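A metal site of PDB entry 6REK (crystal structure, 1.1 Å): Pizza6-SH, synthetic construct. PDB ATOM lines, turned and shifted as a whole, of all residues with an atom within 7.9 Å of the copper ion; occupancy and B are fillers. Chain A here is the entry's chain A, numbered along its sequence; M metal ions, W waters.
The copper ion is bound by a ring nitrogen (NE2) of His 35, a ring nitrogen (ND1) of His 77 and a ring nitrogen (NE2) of His 62. Slightly farther from the copper ion lies water W1 (2.6 Å).
Merely in contact with the copper ion: Thr 60. Of the 14 residues printed, 4 come within 4 Å of the copper ion. Along chain A the residues within 4 Å of the copper ion span positions 35 to 77. The nearest printed residue that does not touch the copper ion is Thr 102 (5.5 Å).
The backbone carbonyl oxygen (O) of His 62 sits at hydrogen-bond distance from the side-chain hydroxyl (OG) of Ser 20. The backbone NH (N) of His 35 is in hydrogen-bond range of the backbone carbonyl oxygen (O) of Thr 18, 3.1 Å away. N of Gly 78 sits at hydrogen-bond distance from OG1 of Thr 60, 2.9 Å away. A ring nitrogen (NE2) of His 77 is in hydrogen-bond range of the side-chain hydroxyl (OG1) of Thr 102 (3.3 Å). The backbone NH (N) of His 62 is in hydrogen-bond range of the backbone carbonyl oxygen (O) of Thr 75. OG1 of Thr 60 sits at hydrogen-bond distance from OD1 of Asn 59 (2.7 Å). The backbone NH of His 77 is in hydrogen-bond range of the backbone carbonyl oxygen of Thr 60, at 3.1 Å.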
ATOM      1  N   THR A  18     -22.936 -13.194 -25.693  1.00  0.00           N
ATOM      2  CA  THR A  18     -22.225 -13.517 -24.443  1.00  0.00           C
ATOM      3  C   THR A  18     -22.662 -14.885 -23.908  1.00  0.00           C
ATOM      4  O   THR A  18     -23.224 -15.004 -22.822  1.00  0.00           O
ATOM      5  CB  THR A  18     -22.334 -12.413 -23.381  1.00  0.00           C
ATOM      6  OG1 THR A  18     -22.029 -11.168 -24.024  1.00  0.00           O
ATOM      7  CG2 THR A  18     -21.339 -12.602 -22.232  1.00  0.00           C
ATOM      8  N   SER A  20     -22.296 -17.880 -21.745  1.00  0.00           N
ATOM      9  CA  SER A  20     -21.639 -17.752 -20.438  1.00  0.00           C
ATOM     10  C   SER A  20     -21.336 -19.072 -19.754  1.00  0.00           C
ATOM     11  O   SER A  20     -20.406 -19.125 -18.926  1.00  0.00           O
ATOM     12  CB  SER A  20     -22.521 -16.916 -19.498  1.00  0.00           C
ATOM     13  OG  SER A  20     -23.815 -17.433 -19.402  1.00  0.00           O
ATOM     14  N   HIS A  35     -26.247 -15.168 -21.978  1.00  0.00           N
ATOM     15  CA  HIS A  35     -26.378 -14.131 -20.945  1.00  0.00           C
ATOM     16  C   HIS A  35     -27.114 -12.891 -21.464  1.00  0.00           C
ATOM     17  O   HIS A  35     -28.049 -12.385 -20.828  1.00  0.00           O
ATOM     18  CB  HIS A  35     -24.982 -13.784 -20.393  1.00  0.00           C
ATOM     19  CG  HIS A  35     -24.936 -12.756 -19.289  1.00  0.00           C
ATOM     20  ND1 HIS A  35     -24.799 -11.406 -19.525  1.00  0.00           N
ATOM     21  CD2 HIS A  35     -24.903 -12.905 -17.939  1.00  0.00           C
ATOM     22  CE1 HIS A  35     -24.671 -10.768 -18.361  1.00  0.00           C
ATOM     23  NE2 HIS A  35     -24.760 -11.651 -17.380  1.00  0.00           N
ATOM     24  N   GLY A  36     -26.691 -12.402 -22.622  1.00  0.00           N
ATOM     25  CA  GLY A  36     -27.236 -11.183 -23.169  1.00  0.00           C
ATOM     26  C   GLY A  36     -28.607 -11.295 -23.761  1.00  0.00           C
ATOM     27  O   GLY A  36     -29.197 -10.252 -24.083  1.00  0.00           O
ATOM     28  N   ASN A  59     -33.329 -13.845 -16.226  1.00  0.00           N
ATOM     29  CA  ASN A  59     -32.476 -12.745 -16.613  1.00  0.00           C
ATOM     30  C   ASN A  59     -31.022 -13.160 -16.537  1.00  0.00           C
ATOM     31  O   ASN A  59     -30.629 -13.920 -15.642  1.00  0.00           O
ATOM     32  CB  ASN A  59     -32.791 -11.528 -15.695  1.00  0.00           C
ATOM     33  CG  ASN A  59     -32.199 -10.222 -16.231  1.00  0.00           C
ATOM     34  OD1 ASN A  59     -31.104  -9.832 -15.922  1.00  0.00           O
ATOM     35  ND2 ASN A  59     -32.957  -9.548 -17.065  1.00  0.00           N
ATOM     36  N   THR A  60     -30.231 -12.679 -17.486  1.00  0.00           N
ATOM     37  CA  THR A  60     -28.774 -12.764 -17.459  1.00  0.00           C
ATOM     38  C   THR A  60     -28.252 -14.056 -16.817  1.00  0.00           C
ATOM     39  O   THR A  60     -27.554 -14.053 -15.781  1.00  0.00           O
ATOM     40  CB  THR A  60     -28.141 -11.522 -16.820  1.00  0.00           C
ATOM     41  OG1 THR A  60     -28.841 -11.186 -15.612  1.00  0.00           O
ATOM     42  CG2 THR A  60     -28.267 -10.331 -17.795  1.00  0.00           C
ATOM     43  N   PRO A  61     -28.473 -15.207 -17.458  1.00  0.00           N
ATOM     44  CA  PRO A  61     -28.007 -16.478 -16.863  1.00  0.00           C
ATOM     45  C   PRO A  61     -26.487 -16.615 -16.995  1.00  0.00           C
ATOM     46  O   PRO A  61     -25.900 -16.217 -17.994  1.00  0.00           O
ATOM     47  CB  PRO A  61     -28.760 -17.525 -17.689  1.00  0.00           C
ATOM     48  CG  PRO A  61     -28.947 -16.858 -19.052  1.00  0.00           C
ATOM     49  CD  PRO A  61     -29.318 -15.430 -18.632  1.00  0.00           C
ATOM     50  N   HIS A  62     -25.853 -17.218 -15.979  1.00  0.00           N
ATOM     51  CA  HIS A  62     -24.425 -17.545 -16.026  1.00  0.00           C
ATOM     52  C   HIS A  62     -24.203 -19.048 -16.132  1.00  0.00           C
ATOM     53  O   HIS A  62     -23.778 -19.579 -17.145  1.00  0.00           O
ATOM     54  CB  HIS A  62     -23.654 -16.981 -14.816  1.00  0.00           C
ATOM     55  CG  HIS A  62     -23.518 -15.480 -14.827  1.00  0.00           C
ATOM     56  ND1 HIS A  62     -22.307 -14.832 -14.721  1.00  0.00           N
ATOM     57  CD2 HIS A  62     -24.454 -14.500 -14.954  1.00  0.00           C
ATOM     58  CE1 HIS A  62     -22.499 -13.532 -14.766  1.00  0.00           C
ATOM     59  NE2 HIS A  62     -23.793 -13.300 -14.889  1.00  0.00           N
ATOM     60  N   THR A  75     -28.165 -20.569 -13.053  1.00  0.00           N
ATOM     61  CA  THR A  75     -28.017 -19.382 -12.206  1.00  0.00           C
ATOM     62  C   THR A  75     -28.468 -18.146 -12.990  1.00  0.00           C
ATOM     63  O   THR A  75     -28.142 -17.993 -14.169  1.00  0.00           O
ATOM     64  CB  THR A  75     -26.575 -19.206 -11.701  1.00  0.00           C
ATOM     65  OG1 THR A  75     -25.696 -18.849 -12.737  1.00  0.00           O
ATOM     66  CG2 THR A  75     -26.096 -20.446 -10.932  1.00  0.00           C
ATOM     67  N   ASP A  76     -29.181 -17.254 -12.299  1.00  0.00           N
ATOM     68  CA  ASP A  76     -29.745 -16.028 -12.836  1.00  0.00           C
ATOM     69  C   ASP A  76     -29.113 -14.847 -12.099  1.00  0.00           C
ATOM     70  O   ASP A  76     -29.250 -14.714 -10.887  1.00  0.00           O
ATOM     71  CB  ASP A  76     -31.271 -16.076 -12.649  1.00  0.00           C
ATOM     72  CG  ASP A  76     -31.994 -14.788 -13.012  1.00  0.00           C
ATOM     73  OD1 ASP A  76     -31.457 -13.668 -12.783  1.00  0.00           O
ATOM     74  OD2 ASP A  76     -33.173 -14.892 -13.488  1.00  0.00           O
ATOM     75  N   HIS A  77     -28.350 -14.043 -12.809  1.00  0.00           N
ATOM     76  CA  HIS A  77     -27.664 -12.913 -12.203  1.00  0.00           C
ATOM     77  C   HIS A  77     -28.631 -11.781 -11.839  1.00  0.00           C
ATOM     78  O   HIS A  77     -28.654 -11.299 -10.713  1.00  0.00           O
ATOM     79  CB  HIS A  77     -26.574 -12.452 -13.188  1.00  0.00           C
ATOM     80  CG  HIS A  77     -25.707 -11.359 -12.692  1.00  0.00           C
ATOM     81  ND1 HIS A  77     -24.826 -10.715 -13.536  1.00  0.00           N
ATOM     82  CD2 HIS A  77     -25.546 -10.802 -11.462  1.00  0.00           C
ATOM     83  CE1 HIS A  77     -24.145  -9.821 -12.844  1.00  0.00           C
ATOM     84  NE2 HIS A  77     -24.585  -9.823 -11.602  1.00  0.00           N
ATOM     85  N   GLY A  78     -29.438 -11.329 -12.813  1.00  0.00           N
ATOM     86  CA  GLY A  78     -30.255 -10.142 -12.563  1.00  0.00           C
ATOM     87  C   GLY A  78     -31.229 -10.311 -11.406  1.00  0.00           C
ATOM     88  O   GLY A  78     -31.517  -9.344 -10.695  1.00  0.00           O
ATOM     89  N   THR A 102     -24.577 -12.333  -7.544  1.00  0.00           N
ATOM     90  CA  THR A 102     -23.891 -12.843  -8.736  1.00  0.00           C
ATOM     91  C   THR A 102     -23.598 -14.335  -8.621  1.00  0.00           C
ATOM     92  O   THR A 102     -22.427 -14.765  -8.595  1.00  0.00           O
ATOM     93  CB  THR A 102     -22.624 -12.054  -9.076  1.00  0.00           C
ATOM     94  OG1 THR A 102     -22.886 -10.661  -8.959  1.00  0.00           O
ATOM     95  CG2 THR A 102     -22.195 -12.315 -10.521  1.00  0.00           C
ATOM     96  N   PRO A 103     -24.629 -15.164  -8.577  1.00  0.00           N
ATOM     97  CA  PRO A 103     -24.381 -16.605  -8.644  1.00  0.00           C
ATOM     98  C   PRO A 103     -23.824 -16.947 -10.036  1.00  0.00           C
ATOM     99  O   PRO A 103     -24.466 -16.691 -11.051  1.00  0.00           O
ATOM    100  CB  PRO A 103     -25.752 -17.227  -8.391  1.00  0.00           C
ATOM    101  CG  PRO A 103     -26.747 -16.149  -8.920  1.00  0.00           C
ATOM    102  CD  PRO A 103     -26.080 -14.839  -8.531  1.00  0.00           C
HETATM  103 CU    CU M   1     -24.540 -11.289 -15.432  1.00  0.00          CU
HETATM  104  O   HOH W   1     -22.214 -10.084 -15.793  1.00  0.00           O
